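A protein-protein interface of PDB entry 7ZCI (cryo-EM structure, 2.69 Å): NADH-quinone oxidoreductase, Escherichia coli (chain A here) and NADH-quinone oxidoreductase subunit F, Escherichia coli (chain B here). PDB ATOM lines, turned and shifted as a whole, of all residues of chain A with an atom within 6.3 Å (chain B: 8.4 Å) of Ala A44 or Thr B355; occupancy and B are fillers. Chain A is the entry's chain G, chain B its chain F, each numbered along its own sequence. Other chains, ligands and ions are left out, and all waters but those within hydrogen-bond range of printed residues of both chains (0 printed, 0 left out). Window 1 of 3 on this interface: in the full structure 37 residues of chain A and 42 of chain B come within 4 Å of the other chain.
The backbone carbonyl oxygen (O) of Gly B352 sits at hydrogen-bond distance from the guanidinium group (NH1) of Arg B358, at 3.0 Å. N of Gly A43 lies within hydrogen-bond range of SD of Met A68 (3.3 Å). The backbone NH (N) of Val A42 lies close to the side-chain sulfur (SD) of Met A68, 3.8 Å away. The guanidinium group of Arg B358 lies close to the backbone carbonyl oxygen of Cys B354, 3.4 Å away. The side-chain sulfur (SG) of Cys A34 lies close to the backbone NH (N) of Ala A44 (3.1 Å). The backbone carbonyl oxygen (O) of Gly A43 lies within hydrogen-bond range of the guanidinium group (NH1) of Arg A46, at 3.2 Å.
O of Thr B396 is in hydrogen-bond range of NH2 of Arg A46, 3.4 Å away. The side-chain hydroxyl (OG1) of Thr B355 lies within hydrogen-bond range of the backbone carbonyl oxygen (O) of Cys A45 (3.0 Å). The side-chain hydroxyl (OH) of Tyr A155 is in hydrogen-bond range of the backbone carbonyl oxygen (O) of Gly B352, 2.7 Å away. O of Lys B395 lies within hydrogen-bond range of NE of Arg A46, 2.8 Å away. NH2 of Arg B358 sits at hydrogen-bond distance from O of Ile A152, 3.1 Å away.
Printed residues of chain A that touch a printed residue of chain B: Val A42, Gly A43, Ala A44, Cys A45, Arg A46, Ser A90, Val A91, Trp A94, Leu A95, Ile A152, Ala A153 and Tyr A155. Of the 19 printed residues of chain B, 14 touch a printed residue of chain A. Hydrophobic or aromatic side chains of chain B within 4 Å of the printed part of chain A: Trp B353, Pro B356, Leu B387, Phe B390, Leu B391 and Phe B397. Among the printed residues, 29 pairs touch across the chains. Among the printed residues, no Asp or Glu carboxylate lies within 4 Å of a Lys or Arg side-chain nitrogen of the other chain.
Among the printed residues, pairs that only touch across the chains: Gly A43 with Phe B397, Ala A44 with Cys B354, Ser A90 with Phe B390, Tyr A155 with Trp B353, Val A42 with Phe B397, Trp A94 with Leu B387, Arg A46 with Pro B356, Trp A94 with Pro B356, Ala A153 with Arg B358, Trp A94 with Asp B359, Ala A44 with Thr B355, Arg A46 with Phe B397, Trp A94 with Phe B390, Ala A44 with Trp B353, Val A42 with Trp B353, Arg A46 with Cys B354, Leu A95 with Thr B355, Trp A94 with Leu B391, Gly A43 with Trp B353, Leu A95 with Asp B359, Trp A94 with Gly B360, Trp A94 with Thr B355, Val A91 with Thr B355 and Leu A95 with Arg B358.
Of the printed residues of chain B, Ala A44 touches Trp B353 (3.7 Å), Cys B354 (3.2 Å) and Thr B355 (3.6 Å). Of chain B, only Trp B353 and Phe B397 come within 4 Å of Gly A43. Of the printed residues of chain A, Leu B391 touches Trp A94 (3.8 Å). Printed residues of chain B within 4 Å of Val A91: Thr B355 (3.97 Å). Ala B401 touches none of the printed residues of chain A. The nearest residue of chain B that does not touch Ala A44 is Phe B397 (5.0 Å). The nearest printed residue of chain B that does not touch Leu A95 is Pro B356 (7.2 Å).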
ATOM      1  N   CYS A  34       8.504 -18.856 -33.894  1.00  0.00           N
ATOM      2  CA  CYS A  34       9.358 -19.208 -35.019  1.00  0.00           C
ATOM      3  C   CYS A  34       8.581 -19.725 -36.221  1.00  0.00           C
ATOM      4  O   CYS A  34       9.064 -19.602 -37.347  1.00  0.00           O
ATOM      5  CB  CYS A  34      10.412 -20.234 -34.591  1.00  0.00           C
ATOM      6  SG  CYS A  34       9.816 -21.863 -34.203  1.00  0.00           S
ATOM      7  N   VAL A  42      10.106 -25.109 -37.928  1.00  0.00           N
ATOM      8  CA  VAL A  42      11.467 -25.488 -37.575  1.00  0.00           C
ATOM      9  C   VAL A  42      11.625 -25.891 -36.117  1.00  0.00           C
ATOM     10  O   VAL A  42      12.626 -26.538 -35.780  1.00  0.00           O
ATOM     11  CB  VAL A  42      12.468 -24.371 -37.930  1.00  0.00           C
ATOM     12  CG1 VAL A  42      12.647 -24.304 -39.426  1.00  0.00           C
ATOM     13  CG2 VAL A  42      12.024 -23.046 -37.359  1.00  0.00           C
ATOM     14  N   GLY A  43      10.683 -25.563 -35.242  1.00  0.00           N
ATOM     15  CA  GLY A  43      10.808 -25.902 -33.837  1.00  0.00           C
ATOM     16  C   GLY A  43      11.882 -25.159 -33.068  1.00  0.00           C
ATOM     17  O   GLY A  43      12.552 -25.759 -32.225  1.00  0.00           O
ATOM     18  N   ALA A  44      12.042 -23.862 -33.312  1.00  0.00           N
ATOM     19  CA  ALA A  44      13.100 -23.098 -32.660  1.00  0.00           C
ATOM     20  C   ALA A  44      12.652 -22.484 -31.337  1.00  0.00           C
ATOM     21  O   ALA A  44      13.200 -22.814 -30.289  1.00  0.00           O
ATOM     22  CB  ALA A  44      13.622 -22.002 -33.594  1.00  0.00           C
ATOM     23  N   CYS A  45      11.643 -21.610 -31.366  1.00  0.00           N
ATOM     24  CA  CYS A  45      11.326 -20.774 -30.210  1.00  0.00           C
ATOM     25  C   CYS A  45      10.796 -21.559 -29.018  1.00  0.00           C
ATOM     26  O   CYS A  45      10.819 -21.043 -27.900  1.00  0.00           O
ATOM     27  CB  CYS A  45      10.311 -19.713 -30.608  1.00  0.00           C
ATOM     28  SG  CYS A  45       8.673 -20.365 -30.954  1.00  0.00           S
ATOM     29  N   ARG A  46      10.324 -22.784 -29.238  1.00  0.00           N
ATOM     30  CA  ARG A  46       9.780 -23.675 -28.210  1.00  0.00           C
ATOM     31  C   ARG A  46       8.577 -23.072 -27.492  1.00  0.00           C
ATOM     32  O   ARG A  46       8.278 -23.441 -26.360  1.00  0.00           O
ATOM     33  CB  ARG A  46      10.828 -24.133 -27.193  1.00  0.00           C
ATOM     34  CG  ARG A  46      12.124 -24.631 -27.796  1.00  0.00           C
ATOM     35  CD  ARG A  46      11.931 -25.705 -28.814  1.00  0.00           C
ATOM     36  NE  ARG A  46      11.600 -26.988 -28.223  1.00  0.00           N
ATOM     37  CZ  ARG A  46      11.503 -28.109 -28.916  1.00  0.00           C
ATOM     38  NH1 ARG A  46      11.731 -28.133 -30.215  1.00  0.00           N
ATOM     39  NH2 ARG A  46      11.158 -29.226 -28.295  1.00  0.00           N
ATOM     40  N   GLN A  47       7.840 -22.193 -28.159  1.00  0.00           N
ATOM     41  CA  GLN A  47       6.704 -21.527 -27.538  1.00  0.00           C
ATOM     42  C   GLN A  47       5.409 -22.309 -27.690  1.00  0.00           C
ATOM     43  O   GLN A  47       4.557 -22.254 -26.803  1.00  0.00           O
ATOM     44  CB  GLN A  47       6.533 -20.126 -28.130  1.00  0.00           C
ATOM     45  CG  GLN A  47       5.475 -19.257 -27.479  1.00  0.00           C
ATOM     46  CD  GLN A  47       5.787 -18.925 -26.045  1.00  0.00           C
ATOM     47  OE1 GLN A  47       6.676 -18.134 -25.761  1.00  0.00           O
ATOM     48  NE2 GLN A  47       5.065 -19.536 -25.132  1.00  0.00           N
ATOM     49  N   CYS A  67       3.867 -27.204 -33.702  1.00  0.00           N
ATOM     50  CA  CYS A  67       4.271 -26.908 -35.067  1.00  0.00           C
ATOM     51  C   CYS A  67       5.078 -28.037 -35.686  1.00  0.00           C
ATOM     52  O   CYS A  67       5.094 -28.167 -36.910  1.00  0.00           O
ATOM     53  CB  CYS A  67       5.057 -25.596 -35.117  1.00  0.00           C
ATOM     54  SG  CYS A  67       6.759 -25.645 -34.545  1.00  0.00           S
ATOM     55  N   MET A  68       5.716 -28.874 -34.874  1.00  0.00           N
ATOM     56  CA  MET A  68       6.503 -30.002 -35.347  1.00  0.00           C
ATOM     57  C   MET A  68       5.776 -31.329 -35.210  1.00  0.00           C
ATOM     58  O   MET A  68       6.404 -32.378 -35.356  1.00  0.00           O
ATOM     59  CB  MET A  68       7.833 -30.071 -34.599  1.00  0.00           C
ATOM     60  CG  MET A  68       8.615 -28.790 -34.614  1.00  0.00           C
ATOM     61  SD  MET A  68       9.190 -28.339 -36.255  1.00  0.00           S
ATOM     62  CE  MET A  68      10.012 -29.842 -36.747  1.00  0.00           C
ATOM     63  N   SER A  90       6.786 -19.873 -19.190  1.00  0.00           N
ATOM     64  CA  SER A  90       8.225 -19.901 -18.947  1.00  0.00           C
ATOM     65  C   SER A  90       9.018 -19.498 -20.184  1.00  0.00           C
ATOM     66  O   SER A  90      10.062 -18.849 -20.074  1.00  0.00           O
ATOM     67  CB  SER A  90       8.648 -21.289 -18.476  1.00  0.00           C
ATOM     68  OG  SER A  90       8.043 -21.610 -17.244  1.00  0.00           O
ATOM     69  N   VAL A  91       8.558 -19.899 -21.368  1.00  0.00           N
ATOM     70  CA  VAL A  91       9.252 -19.508 -22.593  1.00  0.00           C
ATOM     71  C   VAL A  91       9.158 -18.001 -22.800  1.00  0.00           C
ATOM     72  O   VAL A  91      10.146 -17.346 -23.168  1.00  0.00           O
ATOM     73  CB  VAL A  91       8.702 -20.289 -23.802  1.00  0.00           C
ATOM     74  CG1 VAL A  91       9.366 -19.830 -25.074  1.00  0.00           C
ATOM     75  CG2 VAL A  91       8.921 -21.762 -23.611  1.00  0.00           C
ATOM     76  N   VAL A  92       7.979 -17.423 -22.544  1.00  0.00           N
ATOM     77  CA  VAL A  92       7.846 -15.968 -22.624  1.00  0.00           C
ATOM     78  C   VAL A  92       8.736 -15.288 -21.583  1.00  0.00           C
ATOM     79  O   VAL A  92       9.371 -14.267 -21.862  1.00  0.00           O
ATOM     80  CB  VAL A  92       6.365 -15.558 -22.498  1.00  0.00           C
ATOM     81  CG1 VAL A  92       6.214 -14.144 -21.968  1.00  0.00           C
ATOM     82  CG2 VAL A  92       5.698 -15.654 -23.844  1.00  0.00           C
ATOM     83  N   TRP A  94      11.620 -16.430 -20.385  1.00  0.00           N
ATOM     84  CA  TRP A  94      13.001 -16.526 -20.842  1.00  0.00           C
ATOM     85  C   TRP A  94      13.297 -15.516 -21.939  1.00  0.00           C
ATOM     86  O   TRP A  94      14.385 -14.935 -21.973  1.00  0.00           O
ATOM     87  CB  TRP A  94      13.293 -17.940 -21.326  1.00  0.00           C
ATOM     88  CG  TRP A  94      13.378 -18.916 -20.222  1.00  0.00           C
ATOM     89  CD1 TRP A  94      13.915 -18.707 -19.000  1.00  0.00           C
ATOM     90  CD2 TRP A  94      12.907 -20.263 -20.232  1.00  0.00           C
ATOM     91  NE1 TRP A  94      13.810 -19.834 -18.238  1.00  0.00           N
ATOM     92  CE2 TRP A  94      13.192 -20.807 -18.973  1.00  0.00           C
ATOM     93  CE3 TRP A  94      12.264 -21.058 -21.180  1.00  0.00           C
ATOM     94  CZ2 TRP A  94      12.867 -22.111 -18.638  1.00  0.00           C
ATOM     95  CZ3 TRP A  94      11.939 -22.348 -20.843  1.00  0.00           C
ATOM     96  CH2 TRP A  94      12.242 -22.864 -19.585  1.00  0.00           C
ATOM     97  N   LEU A  95      12.344 -15.292 -22.843  1.00  0.00           N
ATOM     98  CA  LEU A  95      12.521 -14.219 -23.818  1.00  0.00           C
ATOM     99  C   LEU A  95      12.498 -12.845 -23.160  1.00  0.00           C
ATOM    100  O   LEU A  95      13.133 -11.910 -23.657  1.00  0.00           O
ATOM    101  CB  LEU A  95      11.447 -14.302 -24.893  1.00  0.00           C
ATOM    102  CG  LEU A  95      11.473 -15.580 -25.717  1.00  0.00           C
ATOM    103  CD1 LEU A  95      10.300 -15.605 -26.653  1.00  0.00           C
ATOM    104  CD2 LEU A  95      12.775 -15.693 -26.478  1.00  0.00           C
ATOM    105  N   ILE A 152      14.378 -11.844 -30.259  1.00  0.00           N
ATOM    106  CA  ILE A 152      14.088 -13.023 -29.463  1.00  0.00           C
ATOM    107  C   ILE A 152      14.686 -14.273 -30.081  1.00  0.00           C
ATOM    108  O   ILE A 152      14.415 -15.376 -29.608  1.00  0.00           O
ATOM    109  CB  ILE A 152      12.581 -13.196 -29.249  1.00  0.00           C
ATOM    110  CG1 ILE A 152      11.874 -13.291 -30.593  1.00  0.00           C
ATOM    111  CG2 ILE A 152      12.038 -12.065 -28.418  1.00  0.00           C
ATOM    112  CD1 ILE A 152      10.466 -13.690 -30.491  1.00  0.00           C
ATOM    113  N   ALA A 153      15.499 -14.115 -31.129  1.00  0.00           N
ATOM    114  CA  ALA A 153      16.179 -15.208 -31.824  1.00  0.00           C
ATOM    115  C   ALA A 153      15.185 -16.274 -32.275  1.00  0.00           C
ATOM    116  O   ALA A 153      15.357 -17.469 -32.045  1.00  0.00           O
ATOM    117  CB  ALA A 153      17.299 -15.802 -30.971  1.00  0.00           C
ATOM    118  N   CYS A 154      14.109 -15.814 -32.897  1.00  0.00           N
ATOM    119  CA  CYS A 154      13.097 -16.701 -33.440  1.00  0.00           C
ATOM    120  C   CYS A 154      13.449 -17.221 -34.830  1.00  0.00           C
ATOM    121  O   CYS A 154      12.764 -18.121 -35.320  1.00  0.00           O
ATOM    122  CB  CYS A 154      11.761 -15.971 -33.478  1.00  0.00           C
ATOM    123  SG  CYS A 154      11.560 -14.918 -34.911  1.00  0.00           S
ATOM    124  N   TYR A 155      14.481 -16.662 -35.467  1.00  0.00           N
ATOM    125  CA  TYR A 155      15.056 -17.059 -36.751  1.00  0.00           C
ATOM    126  C   TYR A 155      14.124 -16.849 -37.933  1.00  0.00           C
ATOM    127  O   TYR A 155      14.424 -17.332 -39.022  1.00  0.00           O
ATOM    128  CB  TYR A 155      15.539 -18.514 -36.747  1.00  0.00           C
ATOM    129  CG  TYR A 155      16.696 -18.763 -35.822  1.00  0.00           C
ATOM    130  CD1 TYR A 155      16.485 -19.077 -34.491  1.00  0.00           C
ATOM    131  CD2 TYR A 155      18.002 -18.671 -36.274  1.00  0.00           C
ATOM    132  CE1 TYR A 155      17.538 -19.294 -33.636  1.00  0.00           C
ATOM    133  CE2 TYR A 155      19.060 -18.890 -35.427  1.00  0.00           C
ATOM    134  CZ  TYR A 155      18.824 -19.198 -34.108  1.00  0.00           C
ATOM    135  OH  TYR A 155      19.869 -19.420 -33.252  1.00  0.00           O
ATOM    136  N   SER B 350      25.930 -23.583 -25.576  1.00  0.00           N
ATOM    137  CA  SER B 350      24.659 -23.584 -26.277  1.00  0.00           C
ATOM    138  C   SER B 350      24.876 -23.168 -27.724  1.00  0.00           C
ATOM    139  O   SER B 350      25.764 -22.377 -28.036  1.00  0.00           O
ATOM    140  CB  SER B 350      23.690 -22.623 -25.593  1.00  0.00           C
ATOM    141  OG  SER B 350      22.430 -22.589 -26.230  1.00  0.00           O
ATOM    142  N   GLY B 352      22.454 -21.775 -29.472  1.00  0.00           N
ATOM    143  CA  GLY B 352      21.643 -20.602 -29.675  1.00  0.00           C
ATOM    144  C   GLY B 352      20.353 -20.822 -30.422  1.00  0.00           C
ATOM    145  O   GLY B 352      19.616 -19.858 -30.633  1.00  0.00           O
ATOM    146  N   TRP B 353      20.048 -22.059 -30.812  1.00  0.00           N
ATOM    147  CA  TRP B 353      18.880 -22.309 -31.649  1.00  0.00           C
ATOM    148  C   TRP B 353      17.586 -22.107 -30.871  1.00  0.00           C
ATOM    149  O   TRP B 353      16.741 -21.297 -31.262  1.00  0.00           O
ATOM    150  CB  TRP B 353      18.953 -23.722 -32.229  1.00  0.00           C
ATOM    151  CG  TRP B 353      17.788 -24.153 -33.067  1.00  0.00           C
ATOM    152  CD1 TRP B 353      16.898 -25.130 -32.772  1.00  0.00           C
ATOM    153  CD2 TRP B 353      17.401 -23.633 -34.343  1.00  0.00           C
ATOM    154  NE1 TRP B 353      15.977 -25.253 -33.771  1.00  0.00           N
ATOM    155  CE2 TRP B 353      16.264 -24.349 -34.754  1.00  0.00           C
ATOM    156  CE3 TRP B 353      17.906 -22.636 -35.180  1.00  0.00           C
ATOM    157  CZ2 TRP B 353      15.616 -24.093 -35.953  1.00  0.00           C
ATOM    158  CZ3 TRP B 353      17.263 -22.388 -36.371  1.00  0.00           C
ATOM    159  CH2 TRP B 353      16.132 -23.114 -36.748  1.00  0.00           C
ATOM    160  N   CYS B 354      17.424 -22.807 -29.756  1.00  0.00           N
ATOM    161  CA  CYS B 354      16.139 -22.864 -29.085  1.00  0.00           C
ATOM    162  C   CYS B 354      16.159 -22.142 -27.742  1.00  0.00           C
ATOM    163  O   CYS B 354      17.164 -22.137 -27.032  1.00  0.00           O
ATOM    164  CB  CYS B 354      15.664 -24.320 -28.950  1.00  0.00           C
ATOM    165  SG  CYS B 354      16.364 -25.371 -27.708  1.00  0.00           S
ATOM    166  N   THR B 355      15.015 -21.526 -27.426  1.00  0.00           N
ATOM    167  CA  THR B 355      14.898 -20.590 -26.307  1.00  0.00           C
ATOM    168  C   THR B 355      15.283 -21.144 -24.937  1.00  0.00           C
ATOM    169  O   THR B 355      16.055 -20.465 -24.244  1.00  0.00           O
ATOM    170  CB  THR B 355      13.473 -20.021 -26.262  1.00  0.00           C
ATOM    171  OG1 THR B 355      13.208 -19.275 -27.451  1.00  0.00           O
ATOM    172  CG2 THR B 355      13.272 -19.122 -25.048  1.00  0.00           C
ATOM    173  N   PRO B 356      14.792 -22.315 -24.470  1.00  0.00           N
ATOM    174  CA  PRO B 356      15.049 -22.686 -23.064  1.00  0.00           C
ATOM    175  C   PRO B 356      16.512 -22.857 -22.722  1.00  0.00           C
ATOM    176  O   PRO B 356      16.965 -22.289 -21.735  1.00  0.00           O
ATOM    177  CB  PRO B 356      14.278 -24.000 -22.905  1.00  0.00           C
ATOM    178  CG  PRO B 356      13.287 -23.976 -23.950  1.00  0.00           C
ATOM    179  CD  PRO B 356      13.978 -23.363 -25.099  1.00  0.00           C
ATOM    180  N   CYS B 357      17.274 -23.568 -23.547  1.00  0.00           N
ATOM    181  CA  CYS B 357      18.710 -23.685 -23.327  1.00  0.00           C
ATOM    182  C   CYS B 357      19.391 -22.324 -23.411  1.00  0.00           C
ATOM    183  O   CYS B 357      19.931 -21.837 -22.409  1.00  0.00           O
ATOM    184  CB  CYS B 357      19.266 -24.677 -24.341  1.00  0.00           C
ATOM    185  SG  CYS B 357      21.008 -24.739 -24.700  1.00  0.00           S
ATOM    186  N   ARG B 358      19.216 -21.634 -24.550  1.00  0.00           N
ATOM    187  CA  ARG B 358      19.891 -20.369 -24.846  1.00  0.00           C
ATOM    188  C   ARG B 358      19.630 -19.290 -23.801  1.00  0.00           C
ATOM    189  O   ARG B 358      20.535 -18.514 -23.474  1.00  0.00           O
ATOM    190  CB  ARG B 358      19.462 -19.867 -26.230  1.00  0.00           C
ATOM    191  CG  ARG B 358      19.677 -18.367 -26.470  1.00  0.00           C
ATOM    192  CD  ARG B 358      19.244 -17.898 -27.832  1.00  0.00           C
ATOM    193  NE  ARG B 358      17.835 -17.538 -27.811  1.00  0.00           N
ATOM    194  CZ  ARG B 358      16.878 -18.265 -28.361  1.00  0.00           C
ATOM    195  NH1 ARG B 358      17.151 -19.369 -29.035  1.00  0.00           N
ATOM    196  NH2 ARG B 358      15.618 -17.878 -28.228  1.00  0.00           N
ATOM    197  N   ASP B 359      18.430 -19.247 -23.237  1.00  0.00           N
ATOM    198  CA  ASP B 359      18.033 -18.156 -22.368  1.00  0.00           C
ATOM    199  C   ASP B 359      17.765 -18.551 -20.927  1.00  0.00           C
ATOM    200  O   ASP B 359      17.592 -17.658 -20.093  1.00  0.00           O
ATOM    201  CB  ASP B 359      16.786 -17.460 -22.930  1.00  0.00           C
ATOM    202  CG  ASP B 359      17.086 -16.639 -24.161  1.00  0.00           C
ATOM    203  OD1 ASP B 359      18.169 -16.025 -24.215  1.00  0.00           O
ATOM    204  OD2 ASP B 359      16.243 -16.604 -25.077  1.00  0.00           O
ATOM    205  N   GLY B 360      17.765 -19.835 -20.590  1.00  0.00           N
ATOM    206  CA  GLY B 360      17.519 -20.252 -19.234  1.00  0.00           C
ATOM    207  C   GLY B 360      18.742 -20.876 -18.615  1.00  0.00           C
ATOM    208  O   GLY B 360      18.864 -20.875 -17.391  1.00  0.00           O
ATOM    209  N   LEU B 361      19.645 -21.445 -19.419  1.00  0.00           N
ATOM    210  CA  LEU B 361      20.945 -21.806 -18.869  1.00  0.00           C
ATOM    211  C   LEU B 361      21.747 -20.602 -18.376  1.00  0.00           C
ATOM    212  O   LEU B 361      22.366 -20.724 -17.307  1.00  0.00           O
ATOM    213  CB  LEU B 361      21.733 -22.643 -19.885  1.00  0.00           C
ATOM    214  CG  LEU B 361      21.308 -24.105 -20.002  1.00  0.00           C
ATOM    215  CD1 LEU B 361      22.260 -24.853 -20.900  1.00  0.00           C
ATOM    216  CD2 LEU B 361      21.251 -24.753 -18.632  1.00  0.00           C
ATOM    217  N   PRO B 362      21.808 -19.451 -19.070  1.00  0.00           N
ATOM    218  CA  PRO B 362      22.440 -18.279 -18.444  1.00  0.00           C
ATOM    219  C   PRO B 362      21.754 -17.806 -17.177  1.00  0.00           C
ATOM    220  O   PRO B 362      22.428 -17.269 -16.292  1.00  0.00           O
ATOM    221  CB  PRO B 362      22.372 -17.219 -19.550  1.00  0.00           C
ATOM    222  CG  PRO B 362      22.357 -17.980 -20.774  1.00  0.00           C
ATOM    223  CD  PRO B 362      21.521 -19.165 -20.489  1.00  0.00           C
ATOM    224  N   LEU B 387      13.796 -24.572 -13.732  1.00  0.00           N
ATOM    225  CA  LEU B 387      14.675 -24.655 -14.894  1.00  0.00           C
ATOM    226  C   LEU B 387      15.051 -26.097 -15.196  1.00  0.00           C
ATOM    227  O   LEU B 387      15.135 -26.493 -16.361  1.00  0.00           O
ATOM    228  CB  LEU B 387      15.930 -23.817 -14.656  1.00  0.00           C
ATOM    229  CG  LEU B 387      15.826 -22.305 -14.847  1.00  0.00           C
ATOM    230  CD1 LEU B 387      17.074 -21.606 -14.339  1.00  0.00           C
ATOM    231  CD2 LEU B 387      15.607 -21.978 -16.301  1.00  0.00           C
ATOM    232  N   PHE B 390      11.871 -27.794 -16.734  1.00  0.00           N
ATOM    233  CA  PHE B 390      11.440 -27.302 -18.031  1.00  0.00           C
ATOM    234  C   PHE B 390      12.529 -27.349 -19.088  1.00  0.00           C
ATOM    235  O   PHE B 390      12.288 -26.921 -20.217  1.00  0.00           O
ATOM    236  CB  PHE B 390      10.902 -25.881 -17.891  1.00  0.00           C
ATOM    237  CG  PHE B 390       9.518 -25.828 -17.330  1.00  0.00           C
ATOM    238  CD1 PHE B 390       8.700 -26.939 -17.385  1.00  0.00           C
ATOM    239  CD2 PHE B 390       9.030 -24.673 -16.757  1.00  0.00           C
ATOM    240  CE1 PHE B 390       7.424 -26.901 -16.880  1.00  0.00           C
ATOM    241  CE2 PHE B 390       7.753 -24.631 -16.247  1.00  0.00           C
ATOM    242  CZ  PHE B 390       6.953 -25.747 -16.307  1.00  0.00           C
ATOM    243  N   LEU B 391      13.709 -27.864 -18.757  1.00  0.00           N
ATOM    244  CA  LEU B 391      14.753 -28.113 -19.740  1.00  0.00           C
ATOM    245  C   LEU B 391      14.995 -29.602 -19.931  1.00  0.00           C
ATOM    246  O   LEU B 391      16.061 -29.998 -20.401  1.00  0.00           O
ATOM    247  CB  LEU B 391      16.046 -27.406 -19.341  1.00  0.00           C
ATOM    248  CG  LEU B 391      16.307 -26.015 -19.915  1.00  0.00           C
ATOM    249  CD1 LEU B 391      15.322 -24.996 -19.387  1.00  0.00           C
ATOM    250  CD2 LEU B 391      17.718 -25.584 -19.610  1.00  0.00           C
ATOM    251  N   LYS B 395      11.551 -30.835 -24.154  1.00  0.00           N
ATOM    252  CA  LYS B 395      11.271 -29.410 -24.074  1.00  0.00           C
ATOM    253  C   LYS B 395      12.202 -28.591 -24.954  1.00  0.00           C
ATOM    254  O   LYS B 395      11.794 -27.553 -25.480  1.00  0.00           O
ATOM    255  CB  LYS B 395      11.360 -28.942 -22.627  1.00  0.00           C
ATOM    256  CG  LYS B 395      10.086 -29.156 -21.841  1.00  0.00           C
ATOM    257  CD  LYS B 395      10.070 -30.470 -21.121  1.00  0.00           C
ATOM    258  CE  LYS B 395       8.821 -30.593 -20.286  1.00  0.00           C
ATOM    259  NZ  LYS B 395       8.783 -31.881 -19.562  1.00  0.00           N
ATOM    260  N   THR B 396      13.439 -29.031 -25.128  1.00  0.00           N
ATOM    261  CA  THR B 396      14.401 -28.336 -25.962  1.00  0.00           C
ATOM    262  C   THR B 396      14.624 -29.102 -27.256  1.00  0.00           C
ATOM    263  O   THR B 396      14.263 -30.275 -27.382  1.00  0.00           O
ATOM    264  CB  THR B 396      15.725 -28.145 -25.224  1.00  0.00           C
ATOM    265  OG1 THR B 396      16.222 -29.417 -24.803  1.00  0.00           O
ATOM    266  CG2 THR B 396      15.521 -27.275 -24.018  1.00  0.00           C
ATOM    267  N   PHE B 397      15.219 -28.408 -28.227  1.00  0.00           N
ATOM    268  CA  PHE B 397      15.342 -28.953 -29.572  1.00  0.00           C
ATOM    269  C   PHE B 397      16.264 -30.166 -29.615  1.00  0.00           C
ATOM    270  O   PHE B 397      15.945 -31.163 -30.266  1.00  0.00           O
ATOM    271  CB  PHE B 397      15.825 -27.866 -30.527  1.00  0.00           C
ATOM    272  CG  PHE B 397      15.735 -28.249 -31.964  1.00  0.00           C
ATOM    273  CD1 PHE B 397      14.533 -28.174 -32.637  1.00  0.00           C
ATOM    274  CD2 PHE B 397      16.849 -28.701 -32.642  1.00  0.00           C
ATOM    275  CE1 PHE B 397      14.448 -28.527 -33.957  1.00  0.00           C
ATOM    276  CE2 PHE B 397      16.762 -29.058 -33.960  1.00  0.00           C
ATOM    277  CZ  PHE B 397      15.564 -28.965 -34.619  1.00  0.00           C
ATOM    278  N   ALA B 401      20.581 -29.452 -23.413  1.00  0.00           N
ATOM    279  CA  ALA B 401      20.019 -28.863 -22.201  1.00  0.00           C
ATOM    280  C   ALA B 401      19.545 -29.873 -21.148  1.00  0.00           C
ATOM    281  O   ALA B 401      19.708 -29.587 -19.953  1.00  0.00           O
ATOM    282  CB  ALA B 401      18.883 -27.904 -22.561  1.00  0.00           C
